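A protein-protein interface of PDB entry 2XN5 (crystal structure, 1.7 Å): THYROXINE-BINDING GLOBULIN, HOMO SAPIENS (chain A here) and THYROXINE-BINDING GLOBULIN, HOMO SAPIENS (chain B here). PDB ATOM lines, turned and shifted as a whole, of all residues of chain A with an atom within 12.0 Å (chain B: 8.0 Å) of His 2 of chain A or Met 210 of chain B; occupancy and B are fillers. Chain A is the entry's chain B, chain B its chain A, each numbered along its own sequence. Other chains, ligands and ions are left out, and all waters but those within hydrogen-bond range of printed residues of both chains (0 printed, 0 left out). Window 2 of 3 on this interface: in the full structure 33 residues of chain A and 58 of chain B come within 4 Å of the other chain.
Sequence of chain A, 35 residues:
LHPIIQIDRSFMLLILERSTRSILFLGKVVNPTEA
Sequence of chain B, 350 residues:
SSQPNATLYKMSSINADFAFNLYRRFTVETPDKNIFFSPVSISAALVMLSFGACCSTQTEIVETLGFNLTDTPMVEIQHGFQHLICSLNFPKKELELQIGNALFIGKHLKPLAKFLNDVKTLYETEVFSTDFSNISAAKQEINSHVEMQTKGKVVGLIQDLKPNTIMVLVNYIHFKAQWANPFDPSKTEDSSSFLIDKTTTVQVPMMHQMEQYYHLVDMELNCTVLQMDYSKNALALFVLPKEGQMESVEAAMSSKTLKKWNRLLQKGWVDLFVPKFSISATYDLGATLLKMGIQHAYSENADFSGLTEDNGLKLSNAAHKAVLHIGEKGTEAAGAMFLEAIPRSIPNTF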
ATOM      1  N   HIS A   2       3.194   2.318  -6.473  1.00  0.00           N
ATOM      2  CA  HIS A   2       1.822   1.772  -6.288  1.00  0.00           C
ATOM      3  C   HIS A   2       1.621   0.521  -7.145  1.00  0.00           C
ATOM      4  O   HIS A   2       2.219   0.408  -8.214  1.00  0.00           O
ATOM      5  CB  HIS A   2       0.780   2.827  -6.662  1.00  0.00           C
ATOM      6  CG  HIS A   2       0.951   4.127  -5.943  1.00  0.00           C
ATOM      7  ND1 HIS A   2       0.949   4.221  -4.567  1.00  0.00           N
ATOM      8  CD2 HIS A   2       1.121   5.387  -6.407  1.00  0.00           C
ATOM      9  CE1 HIS A   2       1.115   5.484  -4.216  1.00  0.00           C
ATOM     10  NE2 HIS A   2       1.220   6.213  -5.313  1.00  0.00           N
ATOM     11  N   PRO A   3       0.761  -0.411  -6.695  1.00  0.00           N
ATOM     12  CA  PRO A   3       0.557  -1.641  -7.462  1.00  0.00           C
ATOM     13  C   PRO A   3      -0.085  -1.399  -8.834  1.00  0.00           C
ATOM     14  O   PRO A   3      -0.992  -0.571  -8.956  1.00  0.00           O
ATOM     15  CB  PRO A   3      -0.382  -2.460  -6.569  1.00  0.00           C
ATOM     16  CG  PRO A   3      -1.084  -1.455  -5.741  1.00  0.00           C
ATOM     17  CD  PRO A   3      -0.054  -0.405  -5.468  1.00  0.00           C
ATOM     18  N   ILE A   4       0.412  -2.111  -9.843  1.00  0.00           N
ATOM     19  CA  ILE A   4      -0.101  -2.020 -11.207  1.00  0.00           C
ATOM     20  C   ILE A   4      -1.135  -3.116 -11.436  1.00  0.00           C
ATOM     21  O   ILE A   4      -0.873  -4.283 -11.166  1.00  0.00           O
ATOM     22  CB  ILE A   4       1.045  -2.178 -12.244  1.00  0.00           C
ATOM     23  CG1 ILE A   4       2.051  -1.023 -12.111  1.00  0.00           C
ATOM     24  CG2 ILE A   4       0.483  -2.245 -13.663  1.00  0.00           C
ATOM     25  CD1 ILE A   4       3.399  -1.270 -12.814  1.00  0.00           C
ATOM     26  N   ILE A   5      -2.321  -2.746 -11.912  1.00  0.00           N
ATOM     27  CA  ILE A   5      -3.294  -3.742 -12.347  1.00  0.00           C
ATOM     28  C   ILE A   5      -3.585  -3.491 -13.816  1.00  0.00           C
ATOM     29  O   ILE A   5      -4.073  -2.426 -14.180  1.00  0.00           O
ATOM     30  CB  ILE A   5      -4.595  -3.713 -11.527  1.00  0.00           C
ATOM     31  CG1 ILE A   5      -4.309  -4.080 -10.061  1.00  0.00           C
ATOM     32  CG2 ILE A   5      -5.611  -4.685 -12.136  1.00  0.00           C
ATOM     33  CD1 ILE A   5      -5.553  -4.046  -9.143  1.00  0.00           C
ATOM     34  N   GLN A   6      -3.231  -4.473 -14.648  1.00  0.00           N
ATOM     35  CA  GLN A   6      -3.401  -4.377 -16.096  1.00  0.00           C
ATOM     36  C   GLN A   6      -4.416  -5.408 -16.554  1.00  0.00           C
ATOM     37  O   GLN A   6      -4.137  -6.607 -16.546  1.00  0.00           O
ATOM     38  CB  GLN A   6      -2.071  -4.633 -16.811  1.00  0.00           C
ATOM     39  CG  GLN A   6      -1.229  -3.407 -17.028  1.00  0.00           C
ATOM     40  CD  GLN A   6       0.087  -3.724 -17.710  1.00  0.00           C
ATOM     41  OE1 GLN A   6       0.910  -4.462 -17.175  1.00  0.00           O
ATOM     42  NE2 GLN A   6       0.297  -3.150 -18.890  1.00  0.00           N
ATOM     43  N   ASN B 181     -14.812   7.897 -10.943  1.00  0.00           N
ATOM     44  CA  ASN B 181     -13.584   8.480 -11.492  1.00  0.00           C
ATOM     45  C   ASN B 181     -13.407   8.214 -12.991  1.00  0.00           C
ATOM     46  O   ASN B 181     -12.830   7.187 -13.376  1.00  0.00           O
ATOM     47  CB  ASN B 181     -12.387   7.958 -10.706  1.00  0.00           C
ATOM     48  CG  ASN B 181     -12.189   8.713  -9.410  1.00  0.00           C
ATOM     49  OD1 ASN B 181     -11.727   9.858  -9.415  1.00  0.00           O
ATOM     50  ND2 ASN B 181     -12.556   8.089  -8.295  1.00  0.00           N
ATOM     51  N   PHE B 183     -12.093   8.216 -16.884  1.00  0.00           N
ATOM     52  CA  PHE B 183     -10.760   8.192 -17.462  1.00  0.00           C
ATOM     53  C   PHE B 183     -10.569   9.412 -18.338  1.00  0.00           C
ATOM     54  O   PHE B 183     -11.524   9.929 -18.921  1.00  0.00           O
ATOM     55  CB  PHE B 183     -10.520   6.921 -18.270  1.00  0.00           C
ATOM     56  CG  PHE B 183     -10.513   5.672 -17.437  1.00  0.00           C
ATOM     57  CD1 PHE B 183      -9.318   5.051 -17.097  1.00  0.00           C
ATOM     58  CD2 PHE B 183     -11.702   5.125 -16.980  1.00  0.00           C
ATOM     59  CE1 PHE B 183      -9.318   3.901 -16.321  1.00  0.00           C
ATOM     60  CE2 PHE B 183     -11.698   3.980 -16.198  1.00  0.00           C
ATOM     61  CZ  PHE B 183     -10.501   3.367 -15.884  1.00  0.00           C
ATOM     62  N   LYS B 187      -5.196  10.067 -22.069  1.00  0.00           N
ATOM     63  CA  LYS B 187      -4.307   9.036 -21.522  1.00  0.00           C
ATOM     64  C   LYS B 187      -4.589   7.638 -22.084  1.00  0.00           C
ATOM     65  O   LYS B 187      -3.851   6.700 -21.809  1.00  0.00           O
ATOM     66  CB  LYS B 187      -4.389   9.010 -19.987  1.00  0.00           C
ATOM     67  CG  LYS B 187      -3.810  10.260 -19.330  1.00  0.00           C
ATOM     68  CD  LYS B 187      -3.576  10.059 -17.839  1.00  0.00           C
ATOM     69  CE  LYS B 187      -2.747  11.196 -17.253  1.00  0.00           C
ATOM     70  NZ  LYS B 187      -3.345  12.526 -17.566  1.00  0.00           N
ATOM     71  N   HIS B 208      -6.230   4.356 -19.007  1.00  0.00           N
ATOM     72  CA  HIS B 208      -5.181   4.349 -17.984  1.00  0.00           C
ATOM     73  C   HIS B 208      -5.452   5.444 -16.969  1.00  0.00           C
ATOM     74  O   HIS B 208      -5.601   6.608 -17.332  1.00  0.00           O
ATOM     75  CB  HIS B 208      -3.805   4.544 -18.659  1.00  0.00           C
ATOM     76  CG  HIS B 208      -2.642   4.619 -17.708  1.00  0.00           C
ATOM     77  ND1 HIS B 208      -1.515   5.366 -17.977  1.00  0.00           N
ATOM     78  CD2 HIS B 208      -2.431   4.046 -16.499  1.00  0.00           C
ATOM     79  CE1 HIS B 208      -0.655   5.240 -16.982  1.00  0.00           C
ATOM     80  NE2 HIS B 208      -1.189   4.451 -16.068  1.00  0.00           N
ATOM     81  N   GLN B 209      -5.538   5.078 -15.692  1.00  0.00           N
ATOM     82  CA  GLN B 209      -5.522   6.096 -14.656  1.00  0.00           C
ATOM     83  C   GLN B 209      -4.971   5.567 -13.350  1.00  0.00           C
ATOM     84  O   GLN B 209      -5.080   4.377 -13.053  1.00  0.00           O
ATOM     85  CB  GLN B 209      -6.908   6.756 -14.498  1.00  0.00           C
ATOM     86  CG  GLN B 209      -7.847   6.167 -13.494  1.00  0.00           C
ATOM     87  CD  GLN B 209      -9.064   7.071 -13.234  1.00  0.00           C
ATOM     88  OE1 GLN B 209      -8.998   8.018 -12.450  1.00  0.00           O
ATOM     89  NE2 GLN B 209     -10.178   6.756 -13.874  1.00  0.00           N
ATOM     90  N   MET B 210      -4.332   6.457 -12.602  1.00  0.00           N
ATOM     91  CA  MET B 210      -3.823   6.122 -11.281  1.00  0.00           C
ATOM     92  C   MET B 210      -4.753   6.758 -10.246  1.00  0.00           C
ATOM     93  O   MET B 210      -4.904   7.986 -10.173  1.00  0.00           O
ATOM     94  CB  MET B 210      -2.373   6.574 -11.133  1.00  0.00           C
ATOM     95  CG  MET B 210      -1.529   5.711 -10.173  1.00  0.00           C
ATOM     96  SD  MET B 210      -1.931   5.950  -8.436  1.00  0.00           S
ATOM     97  CE  MET B 210      -1.541   7.696  -8.250  1.00  0.00           C
ATOM     98  N   GLU B 211      -5.400   5.907  -9.460  1.00  0.00           N
ATOM     99  CA  GLU B 211      -6.450   6.348  -8.583  1.00  0.00           C
ATOM    100  C   GLU B 211      -6.568   5.386  -7.411  1.00  0.00           C
ATOM    101  O   GLU B 211      -6.036   4.271  -7.457  1.00  0.00           O
ATOM    102  CB  GLU B 211      -7.765   6.407  -9.372  1.00  0.00           C
ATOM    103  CG  GLU B 211      -8.913   7.064  -8.672  1.00  0.00           C
ATOM    104  CD  GLU B 211      -8.579   8.458  -8.239  1.00  0.00           C
ATOM    105  OE1 GLU B 211      -8.462   9.329  -9.131  1.00  0.00           O
ATOM    106  OE2 GLU B 211      -8.402   8.676  -7.017  1.00  0.00           O
ATOM    107  N   GLN B 212      -7.235   5.842  -6.360  1.00  0.00           N
ATOM    108  CA  GLN B 212      -7.611   4.980  -5.241  1.00  0.00           C
ATOM    109  C   GLN B 212      -8.830   4.124  -5.607  1.00  0.00           C
ATOM    110  O   GLN B 212      -9.915   4.658  -5.891  1.00  0.00           O
ATOM    111  CB  GLN B 212      -7.884   5.810  -3.977  1.00  0.00           C
ATOM    112  CG  GLN B 212      -6.631   6.451  -3.353  1.00  0.00           C
ATOM    113  CD  GLN B 212      -6.896   7.107  -1.998  1.00  0.00           C
ATOM    114  OE1 GLN B 212      -8.006   7.049  -1.470  1.00  0.00           O
ATOM    115  NE2 GLN B 212      -5.875   7.734  -1.438  1.00  0.00           N
ATOM    116  N   TYR B 213      -8.653   2.801  -5.618  1.00  0.00           N
ATOM    117  CA  TYR B 213      -9.744   1.861  -5.891  1.00  0.00           C
ATOM    118  C   TYR B 213      -9.792   0.801  -4.805  1.00  0.00           C
ATOM    119  O   TYR B 213      -8.747   0.416  -4.278  1.00  0.00           O
ATOM    120  CB  TYR B 213      -9.541   1.129  -7.221  1.00  0.00           C
ATOM    121  CG  TYR B 213      -9.622   1.999  -8.456  1.00  0.00           C
ATOM    122  CD1 TYR B 213     -10.837   2.490  -8.904  1.00  0.00           C
ATOM    123  CD2 TYR B 213      -8.483   2.308  -9.181  1.00  0.00           C
ATOM    124  CE1 TYR B 213     -10.912   3.271 -10.048  1.00  0.00           C
ATOM    125  CE2 TYR B 213      -8.547   3.103 -10.318  1.00  0.00           C
ATOM    126  CZ  TYR B 213      -9.763   3.580 -10.743  1.00  0.00           C
ATOM    127  OH  TYR B 213      -9.830   4.363 -11.878  1.00  0.00           O
ATOM    128  N   HIS B 215      -9.734  -2.826  -4.030  1.00  0.00           N
ATOM    129  CA  HIS B 215      -9.137  -3.959  -4.729  1.00  0.00           C
ATOM    130  C   HIS B 215      -8.656  -5.010  -3.736  1.00  0.00           C
ATOM    131  O   HIS B 215      -8.579  -4.756  -2.537  1.00  0.00           O
ATOM    132  CB  HIS B 215      -7.993  -3.510  -5.658  1.00  0.00           C
ATOM    133  CG  HIS B 215      -6.777  -3.000  -4.943  1.00  0.00           C
ATOM    134  ND1 HIS B 215      -5.598  -3.720  -4.873  1.00  0.00           N
ATOM    135  CD2 HIS B 215      -6.549  -1.843  -4.280  1.00  0.00           C
ATOM    136  CE1 HIS B 215      -4.703  -3.030  -4.188  1.00  0.00           C
ATOM    137  NE2 HIS B 215      -5.251  -1.886  -3.819  1.00  0.00           N
ATOM    138  N   GLY B 268      -7.127   1.579  -2.009  1.00  0.00           N
ATOM    139  CA  GLY B 268      -5.763   2.086  -2.042  1.00  0.00           C
ATOM    140  C   GLY B 268      -5.347   2.415  -3.458  1.00  0.00           C
ATOM    141  O   GLY B 268      -6.077   2.101  -4.413  1.00  0.00           O
ATOM    142  N   TRP B 269      -4.184   3.056  -3.589  1.00  0.00           N
ATOM    143  CA  TRP B 269      -3.654   3.480  -4.895  1.00  0.00           C
ATOM    144  C   TRP B 269      -3.403   2.299  -5.829  1.00  0.00           C
ATOM    145  O   TRP B 269      -2.829   1.298  -5.418  1.00  0.00           O
ATOM    146  CB  TRP B 269      -2.336   4.228  -4.729  1.00  0.00           C
ATOM    147  CG  TRP B 269      -2.454   5.490  -3.965  1.00  0.00           C
ATOM    148  CD1 TRP B 269      -1.972   5.743  -2.719  1.00  0.00           C
ATOM    149  CD2 TRP B 269      -3.111   6.681  -4.397  1.00  0.00           C
ATOM    150  NE1 TRP B 269      -2.277   7.031  -2.347  1.00  0.00           N
ATOM    151  CE2 TRP B 269      -2.988   7.625  -3.356  1.00  0.00           C
ATOM    152  CE3 TRP B 269      -3.795   7.039  -5.561  1.00  0.00           C
ATOM    153  CZ2 TRP B 269      -3.513   8.911  -3.451  1.00  0.00           C
ATOM    154  CZ3 TRP B 269      -4.318   8.323  -5.654  1.00  0.00           C
ATOM    155  CH2 TRP B 269      -4.175   9.237  -4.603  1.00  0.00           C
ATOM    156  N   VAL B 270      -3.834   2.444  -7.080  1.00  0.00           N
ATOM    157  CA  VAL B 270      -3.590   1.457  -8.129  1.00  0.00           C
ATOM    158  C   VAL B 270      -3.271   2.197  -9.426  1.00  0.00           C
ATOM    159  O   VAL B 270      -3.955   3.161  -9.750  1.00  0.00           O
ATOM    160  CB  VAL B 270      -4.836   0.604  -8.360  1.00  0.00           C
ATOM    161  CG1 VAL B 270      -4.651  -0.355  -9.558  1.00  0.00           C
ATOM    162  CG2 VAL B 270      -5.196  -0.139  -7.088  1.00  0.00           C
ATOM    163  N   ASP B 271      -2.230   1.749 -10.123  1.00  0.00           N
ATOM    164  CA  ASP B 271      -1.928   2.168 -11.497  1.00  0.00           C
ATOM    165  C   ASP B 271      -2.734   1.220 -12.406  1.00  0.00           C
ATOM    166  O   ASP B 271      -2.333   0.078 -12.651  1.00  0.00           O
ATOM    167  CB  ASP B 271      -0.405   2.072 -11.752  1.00  0.00           C
ATOM    168  CG  ASP B 271       0.051   2.808 -13.008  1.00  0.00           C
ATOM    169  OD1 ASP B 271      -0.746   3.553 -13.610  1.00  0.00           O
ATOM    170  OD2 ASP B 271       1.235   2.646 -13.390  1.00  0.00           O
ATOM    171  N   LEU B 272      -3.878   1.705 -12.897  1.00  0.00           N
ATOM    172  CA  LEU B 272      -4.871   0.853 -13.549  1.00  0.00           C
ATOM    173  C   LEU B 272      -4.900   1.019 -15.061  1.00  0.00           C
ATOM    174  O   LEU B 272      -4.897   2.141 -15.565  1.00  0.00           O
ATOM    175  CB  LEU B 272      -6.274   1.144 -12.987  1.00  0.00           C
ATOM    176  CG  LEU B 272      -7.453   0.360 -13.565  1.00  0.00           C
ATOM    177  CD1 LEU B 272      -7.336  -1.117 -13.258  1.00  0.00           C
ATOM    178  CD2 LEU B 272      -8.797   0.920 -13.062  1.00  0.00           C
ATOM    179  N   PHE B 273      -4.928  -0.116 -15.760  1.00  0.00           N
ATOM    180  CA  PHE B 273      -5.123  -0.157 -17.209  1.00  0.00           C
ATOM    181  C   PHE B 273      -6.353  -1.027 -17.517  1.00  0.00           C
ATOM    182  O   PHE B 273      -6.414  -2.195 -17.111  1.00  0.00           O
ATOM    183  CB  PHE B 273      -3.882  -0.723 -17.909  1.00  0.00           C
ATOM    184  CG  PHE B 273      -2.636   0.097 -17.721  1.00  0.00           C
ATOM    185  CD1 PHE B 273      -2.221   0.996 -18.701  1.00  0.00           C
ATOM    186  CD2 PHE B 273      -1.856  -0.042 -16.577  1.00  0.00           C
ATOM    187  CE1 PHE B 273      -1.046   1.736 -18.537  1.00  0.00           C
ATOM    188  CE2 PHE B 273      -0.697   0.701 -16.404  1.00  0.00           C
ATOM    189  CZ  PHE B 273      -0.286   1.584 -17.387  1.00  0.00           C
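O of Pro 3 of chain A lies within hydrogen-bond range of N of Asp 271 of chain B. The backbone NH (N) of Ile 5 of chain A lies within hydrogen-bond range of the backbone carbonyl oxygen (O) of Asp 271 of chain B. The backbone NH (N) of Phe 273 of chain B sits at hydrogen-bond distance from the backbone carbonyl oxygen (O) of Ile 5 of chain A (2.9 Å).
A ring nitrogen (NE2) of His 208 of chain B lies within hydrogen-bond range of the side-chain carboxylate of Asp 271 of chain B (2.7 Å). The backbone carbonyl oxygen (O) of Glu 211 of chain B sits at hydrogen-bond distance from the backbone NH (N) of Val 270 of chain B, 2.9 Å away. O of Gln 209 of chain B lies within hydrogen-bond range of N of Leu 272 of chain B, at 2.9 Å.
Met 210 of chain B touches His 2 of chain A. ND1 of His 2 of chain A touches CB of Trp 269 of chain B, at 3.3 Å. CD of Pro 3 of chain A touches O of Trp 269 of chain B, 3.3 Å away. O of Pro 3 of chain A touches CA of Val 270 of chain B, 3.4 Å away. Ile 4 of chain A touches Asp 271 of chain B (CA to O, 3.4 Å). CG1 of Ile 5 of chain A touches CG1 of Val 270 of chain B (3.8 Å). CA of Leu 272 of chain B touches O of Ile 5 of chain A (3.4 Å). Gln 6 of chain A touches Phe 273 of chain B.
Of chain B, only Met 210 and Trp 269 come within 4 Å of His 2 of chain A. Printed residues of chain B within 4 Å of Pro 3 of chain A: Trp 269 (3.3 Å), Val 270 (3.4 Å) and Asp 271 (2.9 Å). Of the printed residues of chain B, Ile 4 of chain A touches Asp 271. Of the printed residues of chain B, Ile 5 of chain A touches Val 270, Asp 271, Leu 272 and Phe 273. Of the printed residues of chain B, Gln 6 of chain A touches Phe 273. Printed residues of chain A within 4 Å of Met 210 of chain B: His 2. Of chain A, only His 2 (3.3 Å) and Pro 3 (3.3 Å) come within 4 Å of Trp 269 of chain B. Val 270 of chain B touches just these residues of chain A: Pro 3 (3.4 Å) and Ile 5 (3.8 Å). Of the printed residues of chain A, Leu 272 of chain B touches Ile 5. Of the printed residues of chain A, Phe 273 of chain B touches Ile 5 (2.9 Å) and Gln 6 (3.5 Å). The nearest residue of chain B that does not touch His 2 of chain A is Val 270 of chain B (4.6 Å). The nearest residue of chain A that does not touch Met 210 of chain B is Pro 3 of chain A (6.4 Å). The nearest printed residue of chain A that does not touch Phe 273 of chain B is Ile 4 of chain A (4.2 Å).
Of the 16 printed residues of chain B, 6 touch a printed residue of chain A. Printed residues of chain B that touch a printed residue of chain A: Met 210, Trp 269, Val 270, Asp 271, Leu 272 and Phe 273. Of the 5 printed residues of chain A, 5 touch a printed residue of chain B. Hydrophobic or aromatic side chains of chain A that line the printed part of chain B: His 2, Pro 3, Ile 4 and Ile 5. Along chain A the printed residues that touch a printed residue of chain B span positions 2 to 6. Among the printed residues, 11 pairs touch across the chains.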
